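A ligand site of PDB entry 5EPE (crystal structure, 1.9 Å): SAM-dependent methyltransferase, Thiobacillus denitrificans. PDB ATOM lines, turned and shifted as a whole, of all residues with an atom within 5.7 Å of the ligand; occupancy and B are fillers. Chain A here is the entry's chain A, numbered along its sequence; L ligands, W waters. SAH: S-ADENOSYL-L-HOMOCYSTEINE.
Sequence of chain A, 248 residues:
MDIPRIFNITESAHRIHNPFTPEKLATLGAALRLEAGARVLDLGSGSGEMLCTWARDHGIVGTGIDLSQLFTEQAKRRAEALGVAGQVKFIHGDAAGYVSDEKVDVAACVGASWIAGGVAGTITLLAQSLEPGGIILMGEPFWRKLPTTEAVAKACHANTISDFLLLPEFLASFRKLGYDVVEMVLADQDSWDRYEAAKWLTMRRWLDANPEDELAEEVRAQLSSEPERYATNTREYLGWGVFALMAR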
ATOM      1  N   ILE A   3       8.663  -2.426 -20.254  1.00  0.00           N
ATOM      2  CA  ILE A   3       7.627  -3.404 -19.889  1.00  0.00           C
ATOM      3  C   ILE A   3       8.318  -4.613 -19.239  1.00  0.00           C
ATOM      4  O   ILE A   3       9.536  -4.770 -19.353  1.00  0.00           O
ATOM      5  CB  ILE A   3       6.743  -3.755 -21.107  1.00  0.00           C
ATOM      6  CG1 ILE A   3       7.527  -4.568 -22.163  1.00  0.00           C
ATOM      7  CG2 ILE A   3       6.150  -2.480 -21.723  1.00  0.00           C
ATOM      8  CD1 ILE A   3       6.616  -5.107 -23.262  1.00  0.00           C
ATOM      9  N   GLU A  11       7.314 -12.186 -26.895  1.00  0.00           N
ATOM     10  CA  GLU A  11       6.911 -11.523 -28.128  1.00  0.00           C
ATOM     11  C   GLU A  11       8.048 -10.930 -28.950  1.00  0.00           C
ATOM     12  O   GLU A  11       7.805 -10.148 -29.878  1.00  0.00           O
ATOM     13  CB  GLU A  11       5.862 -10.478 -27.800  1.00  0.00           C
ATOM     14  CG  GLU A  11       4.596 -11.149 -27.262  1.00  0.00           C
ATOM     15  CD  GLU A  11       3.359 -10.287 -27.250  1.00  0.00           C
ATOM     16  OE1 GLU A  11       2.468 -10.570 -26.442  1.00  0.00           O
ATOM     17  OE2 GLU A  11       3.265  -9.334 -28.021  1.00  0.00           O
ATOM     18  N   ARG A  15       5.862  -9.254 -35.175  1.00  0.00           N
ATOM     19  CA  ARG A  15       5.720  -7.918 -35.788  1.00  0.00           C
ATOM     20  C   ARG A  15       4.444  -7.250 -35.282  1.00  0.00           C
ATOM     21  O   ARG A  15       4.454  -6.070 -35.036  1.00  0.00           O
ATOM     22  CB  ARG A  15       5.689  -7.997 -37.306  1.00  0.00           C
ATOM     23  CG  ARG A  15       7.063  -8.345 -37.898  1.00  0.00           C
ATOM     24  CD  ARG A  15       6.931  -8.404 -39.412  1.00  0.00           C
ATOM     25  NE  ARG A  15       8.216  -8.780 -40.007  1.00  0.00           N
ATOM     26  CZ  ARG A  15       8.367  -9.335 -41.190  1.00  0.00           C
ATOM     27  NH1 ARG A  15       7.341  -9.576 -41.979  1.00  0.00           N
ATOM     28  NH2 ARG A  15       9.578  -9.632 -41.618  1.00  0.00           N
ATOM     29  N   ILE A  16       3.395  -8.023 -35.061  1.00  0.00           N
ATOM     30  CA  ILE A  16       2.104  -7.532 -34.608  1.00  0.00           C
ATOM     31  C   ILE A  16       1.814  -8.149 -33.240  1.00  0.00           C
ATOM     32  O   ILE A  16       1.753  -9.352 -33.108  1.00  0.00           O
ATOM     33  CB  ILE A  16       0.994  -7.892 -35.629  1.00  0.00           C
ATOM     34  CG1 ILE A  16       1.336  -7.351 -37.019  1.00  0.00           C
ATOM     35  CG2 ILE A  16      -0.367  -7.406 -35.118  1.00  0.00           C
ATOM     36  CD1 ILE A  16       0.537  -7.912 -38.183  1.00  0.00           C
ATOM     37  N   HIS A  17       1.693  -7.307 -32.209  1.00  0.00           N
ATOM     38  CA  HIS A  17       1.494  -7.723 -30.866  1.00  0.00           C
ATOM     39  C   HIS A  17      -0.004  -7.749 -30.511  1.00  0.00           C
ATOM     40  O   HIS A  17      -0.414  -7.244 -29.463  1.00  0.00           O
ATOM     41  CB  HIS A  17       2.257  -6.771 -29.918  1.00  0.00           C
ATOM     42  CG  HIS A  17       3.735  -6.717 -30.187  1.00  0.00           C
ATOM     43  ND1 HIS A  17       4.602  -7.638 -29.666  1.00  0.00           N
ATOM     44  CD2 HIS A  17       4.475  -5.906 -30.975  1.00  0.00           C
ATOM     45  CE1 HIS A  17       5.838  -7.369 -30.101  1.00  0.00           C
ATOM     46  NE2 HIS A  17       5.779  -6.322 -30.898  1.00  0.00           N
ATOM     47  N   ASN A  18      -0.781  -8.406 -31.342  1.00  0.00           N
ATOM     48  CA  ASN A  18      -2.203  -8.469 -31.182  1.00  0.00           C
ATOM     49  C   ASN A  18      -2.684  -9.560 -32.123  1.00  0.00           C
ATOM     50  O   ASN A  18      -1.977  -9.945 -33.044  1.00  0.00           O
ATOM     51  CB  ASN A  18      -2.852  -7.124 -31.563  1.00  0.00           C
ATOM     52  CG  ASN A  18      -3.038  -6.206 -30.376  1.00  0.00           C
ATOM     53  OD1 ASN A  18      -3.583  -6.609 -29.335  1.00  0.00           O
ATOM     54  ND2 ASN A  18      -2.648  -4.966 -30.524  1.00  0.00           N
ATOM     55  N   ASP A  42       0.046   6.958 -33.106  1.00  0.00           N
ATOM     56  CA  ASP A  42      -0.186   5.574 -32.595  1.00  0.00           C
ATOM     57  C   ASP A  42       0.387   5.496 -31.183  1.00  0.00           C
ATOM     58  O   ASP A  42       1.599   5.559 -30.986  1.00  0.00           O
ATOM     59  CB  ASP A  42       0.430   4.546 -33.528  1.00  0.00           C
ATOM     60  CG  ASP A  42      -0.034   3.104 -33.237  1.00  0.00           C
ATOM     61  OD1 ASP A  42      -1.004   2.864 -32.426  1.00  0.00           O
ATOM     62  OD2 ASP A  42       0.583   2.184 -33.878  1.00  0.00           O
ATOM     63  N   LEU A  43      -0.490   5.418 -30.189  1.00  0.00           N
ATOM     64  CA  LEU A  43      -0.054   5.278 -28.786  1.00  0.00           C
ATOM     65  C   LEU A  43      -0.013   3.794 -28.366  1.00  0.00           C
ATOM     66  O   LEU A  43      -1.047   3.109 -28.351  1.00  0.00           O
ATOM     67  CB  LEU A  43      -0.996   6.020 -27.859  1.00  0.00           C
ATOM     68  CG  LEU A  43      -1.137   7.508 -28.157  1.00  0.00           C
ATOM     69  CD1 LEU A  43      -1.935   8.196 -27.069  1.00  0.00           C
ATOM     70  CD2 LEU A  43       0.228   8.189 -28.281  1.00  0.00           C
ATOM     71  N   GLY A  44       1.168   3.333 -27.965  1.00  0.00           N
ATOM     72  CA  GLY A  44       1.418   1.920 -27.724  1.00  0.00           C
ATOM     73  C   GLY A  44       1.626   1.203 -29.029  1.00  0.00           C
ATOM     74  O   GLY A  44       0.962   0.178 -29.327  1.00  0.00           O
ATOM     75  N   SER A  45       2.582   1.740 -29.814  1.00  0.00           N
ATOM     76  CA  SER A  45       2.780   1.344 -31.192  1.00  0.00           C
ATOM     77  C   SER A  45       3.522   0.002 -31.437  1.00  0.00           C
ATOM     78  O   SER A  45       3.683  -0.407 -32.590  1.00  0.00           O
ATOM     79  CB  SER A  45       3.414   2.482 -31.982  1.00  0.00           C
ATOM     80  OG  SER A  45       4.586   2.906 -31.377  1.00  0.00           O
ATOM     81  N   GLY A  46       3.947  -0.675 -30.380  1.00  0.00           N
ATOM     82  CA  GLY A  46       4.549  -1.985 -30.485  1.00  0.00           C
ATOM     83  C   GLY A  46       5.807  -1.920 -31.304  1.00  0.00           C
ATOM     84  O   GLY A  46       6.682  -1.058 -31.043  1.00  0.00           O
ATOM     85  N   SER A  47       5.885  -2.798 -32.303  1.00  0.00           N
ATOM     86  CA  SER A  47       7.042  -2.906 -33.174  1.00  0.00           C
ATOM     87  C   SER A  47       6.847  -2.110 -34.480  1.00  0.00           C
ATOM     88  O   SER A  47       7.561  -2.322 -35.469  1.00  0.00           O
ATOM     89  CB  SER A  47       7.428  -4.382 -33.388  1.00  0.00           C
ATOM     90  OG  SER A  47       7.892  -4.973 -32.167  1.00  0.00           O
ATOM     91  N   ILE A  65       4.460   5.912 -30.211  1.00  0.00           N
ATOM     92  CA  ILE A  65       5.078   5.948 -28.886  1.00  0.00           C
ATOM     93  C   ILE A  65       4.895   4.605 -28.236  1.00  0.00           C
ATOM     94  O   ILE A  65       3.751   4.083 -28.165  1.00  0.00           O
ATOM     95  CB  ILE A  65       4.397   6.971 -27.936  1.00  0.00           C
ATOM     96  CG1 ILE A  65       4.080   8.316 -28.578  1.00  0.00           C
ATOM     97  CG2 ILE A  65       5.220   7.162 -26.683  1.00  0.00           C
ATOM     98  CD1 ILE A  65       5.197   8.958 -29.303  1.00  0.00           C
ATOM     99  N   ASP A  66       5.982   4.038 -27.722  1.00  0.00           N
ATOM    100  CA  ASP A  66       5.909   2.767 -27.048  1.00  0.00           C
ATOM    101  C   ASP A  66       6.860   2.712 -25.871  1.00  0.00           C
ATOM    102  O   ASP A  66       8.011   3.221 -25.933  1.00  0.00           O
ATOM    103  CB  ASP A  66       6.162   1.575 -27.982  1.00  0.00           C
ATOM    104  CG  ASP A  66       5.604   0.251 -27.408  1.00  0.00           C
ATOM    105  OD1 ASP A  66       4.404  -0.033 -27.644  1.00  0.00           O
ATOM    106  OD2 ASP A  66       6.354  -0.497 -26.687  1.00  0.00           O
ATOM    107  N   LEU A  67       6.387   2.073 -24.796  1.00  0.00           N
ATOM    108  CA  LEU A  67       7.160   1.939 -23.564  1.00  0.00           C
ATOM    109  C   LEU A  67       8.286   0.886 -23.649  1.00  0.00           C
ATOM    110  O   LEU A  67       9.242   0.928 -22.848  1.00  0.00           O
ATOM    111  CB  LEU A  67       6.206   1.541 -22.425  1.00  0.00           C
ATOM    112  CG  LEU A  67       6.714   1.565 -20.997  1.00  0.00           C
ATOM    113  CD1 LEU A  67       7.298   2.927 -20.703  1.00  0.00           C
ATOM    114  CD2 LEU A  67       5.590   1.211 -20.016  1.00  0.00           C
ATOM    115  N   SER A  68       8.180  -0.069 -24.573  1.00  0.00           N
ATOM    116  CA  SER A  68       9.206  -1.111 -24.696  1.00  0.00           C
ATOM    117  C   SER A  68      10.428  -0.587 -25.483  1.00  0.00           C
ATOM    118  O   SER A  68      10.310  -0.090 -26.620  1.00  0.00           O
ATOM    119  CB  SER A  68       8.653  -2.342 -25.438  1.00  0.00           C
ATOM    120  OG  SER A  68       9.711  -3.251 -25.715  1.00  0.00           O
ATOM    121  N   PHE A  71      10.885  -3.152 -28.500  1.00  0.00           N
ATOM    122  CA  PHE A  71       9.912  -2.993 -29.596  1.00  0.00           C
ATOM    123  C   PHE A  71      10.136  -1.653 -30.332  1.00  0.00           C
ATOM    124  O   PHE A  71       9.991  -1.586 -31.552  1.00  0.00           O
ATOM    125  CB  PHE A  71       8.451  -3.103 -29.132  1.00  0.00           C
ATOM    126  CG  PHE A  71       8.071  -4.378 -28.383  1.00  0.00           C
ATOM    127  CD1 PHE A  71       8.821  -5.565 -28.495  1.00  0.00           C
ATOM    128  CD2 PHE A  71       6.918  -4.389 -27.593  1.00  0.00           C
ATOM    129  CE1 PHE A  71       8.453  -6.714 -27.788  1.00  0.00           C
ATOM    130  CE2 PHE A  71       6.533  -5.551 -26.894  1.00  0.00           C
ATOM    131  CZ  PHE A  71       7.323  -6.702 -26.978  1.00  0.00           C
ATOM    132  N   GLY A  93       8.976   5.678 -24.868  1.00  0.00           N
ATOM    133  CA  GLY A  93       8.447   6.382 -23.699  1.00  0.00           C
ATOM    134  C   GLY A  93       7.022   6.042 -23.308  1.00  0.00           C
ATOM    135  O   GLY A  93       6.374   5.227 -23.934  1.00  0.00           O
ATOM    136  N   ASP A  94       6.554   6.690 -22.241  1.00  0.00           N
ATOM    137  CA  ASP A  94       5.229   6.477 -21.680  1.00  0.00           C
ATOM    138  C   ASP A  94       4.254   7.352 -22.435  1.00  0.00           C
ATOM    139  O   ASP A  94       4.430   8.559 -22.469  1.00  0.00           O
ATOM    140  CB  ASP A  94       5.254   6.875 -20.206  1.00  0.00           C
ATOM    141  CG  ASP A  94       3.984   6.458 -19.445  1.00  0.00           C
ATOM    142  OD1 ASP A  94       2.950   6.128 -20.048  1.00  0.00           O
ATOM    143  OD2 ASP A  94       4.046   6.467 -18.179  1.00  0.00           O
ATOM    144  N   ALA A  95       3.214   6.764 -23.017  1.00  0.00           N
ATOM    145  CA  ALA A  95       2.241   7.520 -23.792  1.00  0.00           C
ATOM    146  C   ALA A  95       1.077   8.131 -22.971  1.00  0.00           C
ATOM    147  O   ALA A  95       0.200   8.829 -23.529  1.00  0.00           O
ATOM    148  CB  ALA A  95       1.681   6.640 -24.889  1.00  0.00           C
ATOM    149  N   ALA A  96       1.024   7.851 -21.674  1.00  0.00           N
ATOM    150  CA  ALA A  96       0.009   8.442 -20.821  1.00  0.00           C
ATOM    151  C   ALA A  96       0.031   9.965 -20.933  1.00  0.00           C
ATOM    152  O   ALA A  96       1.087  10.595 -20.864  1.00  0.00           O
ATOM    153  CB  ALA A  96       0.233   8.031 -19.366  1.00  0.00           C
ATOM    154  N   VAL A 110      -4.125   0.778 -30.241  1.00  0.00           N
ATOM    155  CA  VAL A 110      -4.472  -0.548 -30.661  1.00  0.00           C
ATOM    156  C   VAL A 110      -4.017  -1.553 -29.593  1.00  0.00           C
ATOM    157  O   VAL A 110      -2.919  -2.085 -29.623  1.00  0.00           O
ATOM    158  CB  VAL A 110      -3.916  -0.811 -32.050  1.00  0.00           C
ATOM    159  CG1 VAL A 110      -4.341  -2.211 -32.568  1.00  0.00           C
ATOM    160  CG2 VAL A 110      -4.441   0.252 -33.014  1.00  0.00           C
ATOM    161  N   GLY A 111      -4.879  -1.766 -28.641  1.00  0.00           N
ATOM    162  CA  GLY A 111      -4.672  -2.722 -27.541  1.00  0.00           C
ATOM    163  C   GLY A 111      -3.772  -2.211 -26.443  1.00  0.00           C
ATOM    164  O   GLY A 111      -2.908  -2.945 -25.946  1.00  0.00           O
ATOM    165  N   ALA A 112      -3.872  -0.934 -26.106  1.00  0.00           N
ATOM    166  CA  ALA A 112      -3.087  -0.387 -24.992  1.00  0.00           C
ATOM    167  C   ALA A 112      -3.889   0.637 -24.199  1.00  0.00           C
ATOM    168  O   ALA A 112      -3.325   1.566 -23.645  1.00  0.00           O
ATOM    169  CB  ALA A 112      -1.791   0.183 -25.491  1.00  0.00           C
ATOM    170  N   TRP A 114      -5.197   0.839 -21.243  1.00  0.00           N
ATOM    171  CA  TRP A 114      -4.869   1.122 -19.834  1.00  0.00           C
ATOM    172  C   TRP A 114      -4.011   2.407 -19.679  1.00  0.00           C
ATOM    173  O   TRP A 114      -3.920   2.952 -18.605  1.00  0.00           O
ATOM    174  CB  TRP A 114      -4.148  -0.066 -19.186  1.00  0.00           C
ATOM    175  CG  TRP A 114      -2.911  -0.429 -19.915  1.00  0.00           C
ATOM    176  CD1 TRP A 114      -1.694   0.222 -19.853  1.00  0.00           C
ATOM    177  CD2 TRP A 114      -2.770  -1.475 -20.905  1.00  0.00           C
ATOM    178  NE1 TRP A 114      -0.793  -0.408 -20.706  1.00  0.00           N
ATOM    179  CE2 TRP A 114      -1.418  -1.449 -21.353  1.00  0.00           C
ATOM    180  CE3 TRP A 114      -3.645  -2.426 -21.435  1.00  0.00           C
ATOM    181  CZ2 TRP A 114      -0.931  -2.325 -22.329  1.00  0.00           C
ATOM    182  CZ3 TRP A 114      -3.156  -3.325 -22.403  1.00  0.00           C
ATOM    183  CH2 TRP A 114      -1.810  -3.265 -22.838  1.00  0.00           C
ATOM    184  N   ILE A 115      -3.359   2.842 -20.750  1.00  0.00           N
ATOM    185  CA  ILE A 115      -2.640   4.105 -20.813  1.00  0.00           C
ATOM    186  C   ILE A 115      -3.447   5.291 -20.279  1.00  0.00           C
ATOM    187  O   ILE A 115      -2.906   6.172 -19.605  1.00  0.00           O
ATOM    188  CB  ILE A 115      -2.179   4.275 -22.287  1.00  0.00           C
ATOM    189  CG1 ILE A 115      -0.816   3.614 -22.449  1.00  0.00           C
ATOM    190  CG2 ILE A 115      -2.236   5.660 -22.835  1.00  0.00           C
ATOM    191  CD1 ILE A 115      -0.488   3.284 -23.867  1.00  0.00           C
ATOM    192  N   TRP A 240     -11.738  -9.971 -30.707  1.00  0.00           N
ATOM    193  CA  TRP A 240     -10.864  -8.796 -30.734  1.00  0.00           C
ATOM    194  C   TRP A 240     -11.070  -8.071 -32.065  1.00  0.00           C
ATOM    195  O   TRP A 240     -11.433  -8.677 -33.112  1.00  0.00           O
ATOM    196  CB  TRP A 240      -9.394  -9.177 -30.512  1.00  0.00           C
ATOM    197  CG  TRP A 240      -8.503  -8.042 -30.170  1.00  0.00           C
ATOM    198  CD1 TRP A 240      -8.163  -7.596 -28.911  1.00  0.00           C
ATOM    199  CD2 TRP A 240      -7.763  -7.237 -31.090  1.00  0.00           C
ATOM    200  NE1 TRP A 240      -7.356  -6.498 -29.018  1.00  0.00           N
ATOM    201  CE2 TRP A 240      -7.047  -6.303 -30.341  1.00  0.00           C
ATOM    202  CE3 TRP A 240      -7.644  -7.231 -32.498  1.00  0.00           C
ATOM    203  CZ2 TRP A 240      -6.199  -5.347 -30.948  1.00  0.00           C
ATOM    204  CZ3 TRP A 240      -6.850  -6.296 -33.121  1.00  0.00           C
ATOM    205  CH2 TRP A 240      -6.126  -5.354 -32.341  1.00  0.00           C
HETATM  206  N   SAH L   1      -0.305  -1.589 -31.100  1.00  0.00           N
HETATM  207  CA  SAH L   1       0.835  -2.585 -31.101  1.00  0.00           C
HETATM  208  CB  SAH L   1       1.160  -3.026 -29.690  1.00  0.00           C
HETATM  209  CG  SAH L   1       0.033  -3.698 -28.875  1.00  0.00           C
HETATM  210  SD  SAH L   1       0.626  -4.513 -27.414  1.00  0.00           S
HETATM  211  C   SAH L   1       0.546  -3.791 -31.973  1.00  0.00           C
HETATM  212  O   SAH L   1      -0.629  -4.072 -32.262  1.00  0.00           O
HETATM  213  OXT SAH L   1       1.472  -4.510 -32.411  1.00  0.00           O
HETATM  214  C5' SAH L   1       0.596  -3.264 -26.098  1.00  0.00           C
HETATM  215  C4' SAH L   1       1.768  -2.295 -26.257  1.00  0.00           C
HETATM  216  O4' SAH L   1       1.647  -1.213 -25.307  1.00  0.00           O
HETATM  217  C3' SAH L   1       3.159  -2.926 -26.026  1.00  0.00           C
HETATM  218  O3' SAH L   1       3.959  -2.680 -27.190  1.00  0.00           O
HETATM  219  C2' SAH L   1       3.727  -2.205 -24.802  1.00  0.00           C
HETATM  220  O2' SAH L   1       5.126  -1.950 -24.914  1.00  0.00           O
HETATM  221  C1' SAH L   1       2.978  -0.904 -24.852  1.00  0.00           C
HETATM  222  N9  SAH L   1       2.800  -0.110 -23.636  1.00  0.00           N
HETATM  223  C8  SAH L   1       2.415  -0.564 -22.405  1.00  0.00           C
HETATM  224  N7  SAH L   1       2.280   0.440 -21.551  1.00  0.00           N
HETATM  225  C5  SAH L   1       2.598   1.589 -22.293  1.00  0.00           C
HETATM  226  C6  SAH L   1       2.671   2.968 -21.958  1.00  0.00           C
HETATM  227  N6  SAH L   1       2.367   3.390 -20.707  1.00  0.00           N
HETATM  228  N1  SAH L   1       3.007   3.866 -22.914  1.00  0.00           N
HETATM  229  C2  SAH L   1       3.311   3.411 -24.148  1.00  0.00           C
HETATM  230  N3  SAH L   1       3.299   2.128 -24.563  1.00  0.00           N
HETATM  231  C4  SAH L   1       2.920   1.247 -23.580  1.00  0.00           C
HETATM  232  O   HOH W   1       0.458  -3.909 -35.588  1.00  0.00           O
HETATM  233  O   HOH W   2       3.780  -3.635 -33.923  1.00  0.00           O
HETATM  234  O   HOH W   3      -0.193  -0.312 -33.504  1.00  0.00           O
HETATM  235  O   HOH W   4      -1.449   1.259 -30.686  1.00  0.00           O
HETATM  236  O   HOH W   5       1.238   1.903 -18.463  1.00  0.00           O
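The backbone NH (N) of His 17 sits at hydrogen-bond distance from an oxygen (OXT) of the ligand (2.8 Å).
The side-chain amide nitrogen (ND2) of Asn 18 is in hydrogen-bond range of an oxygen (O) of the ligand.
A nitrogen (N) of the ligand is in hydrogen-bond range of the backbone carbonyl oxygen (O) of Val 110.
The side-chain carboxylate (OD2) of Asp 66 lies within hydrogen-bond range of an oxygen (O2') of the ligand, 2.6 Å away.
A nitrogen (N) of the ligand sits at hydrogen-bond distance from the backbone carbonyl oxygen (O) of Gly 44 (2.8 Å).
N1 of the ligand is in hydrogen-bond range of N of Ala 95, 2.9 Å away.
N of Leu 67 sits at hydrogen-bond distance from N3 of the ligand, 3.1 Å away.
The indole nitrogen (NE1) of Trp 114 is in hydrogen-bond range of a nitrogen (N7) of the ligand, at 3.3 Å.
The side-chain carboxylate of Asp 94 is in hydrogen-bond range of a nitrogen (N6) of the ligand (2.9 Å).
The backbone NH (N) of Leu 67 lies within hydrogen-bond range of the backbone carbonyl oxygen (O) of Gly 93, at 3.3 Å.
N of Gly 44 lies within hydrogen-bond range of O of Ile 65, at 2.7 Å.
OD2 of Asp 66 sits at hydrogen-bond distance from N of Ser 68, at 2.8 Å.
O of Ile 65 lies within hydrogen-bond range of N of Ser 45, 3.1 Å away.
The side-chain amide nitrogen (ND2) of Asn 18 is in hydrogen-bond range of the backbone carbonyl oxygen (O) of Val 110 (3.0 Å).
The backbone NH (N) of Gly 46 lies within hydrogen-bond range of the side-chain carboxylate (OD1) of Asp 66, at 2.8 Å.
The side-chain carboxylate (OE2) of Glu 11 sits at hydrogen-bond distance from a ring nitrogen (ND1) of His 17 (2.7 Å).
The side-chain carboxylate (OD1) of Asp 66 is in hydrogen-bond range of the backbone NH (N) of Ser 45 (3.3 Å).
Merely in contact with the ligand: Ile 3 (3.4 Å), Gly 46 (3.4 Å), Phe 71 (3.4 Å), Gly 111 (3.5 Å), Gly 93 (3.6 Å), Ile 115 (3.6 Å), Ser 68 (3.6 Å), Ala 112 (3.7 Å), Ser 45 (3.7 Å) and Ile 16 (3.7 Å).
Hydrophobic or aromatic side chains that line the ligand: Ile 3, His 17, Leu 67, Phe 71, Ala 95, Val 110, Ala 112, Trp 114 and Ile 115.
Within 4 Å of the ligand: Ile 3, Ile 16, His 17, Asn 18, Gly 44, Ser 45, Gly 46, Asp 66, Leu 67, Ser 68, Phe 71, Gly 93, Asp 94, Ala 95, Val 110, Gly 111, Ala 112, Trp 114 and Ile 115.
The nearest printed residue that does not touch the ligand is Ile 65 (4.1 Å).
Water W3 bridges OD2 of Asp 42 (2.6 Å) and N of the ligand (2.7 Å).
Water W2 lies within hydrogen-bond range of O of Arg 15 (2.8 Å), N of Ser 47 (2.8 Å), OXT of the ligand (2.9 Å) and O of Ser 45 (3.5 Å).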
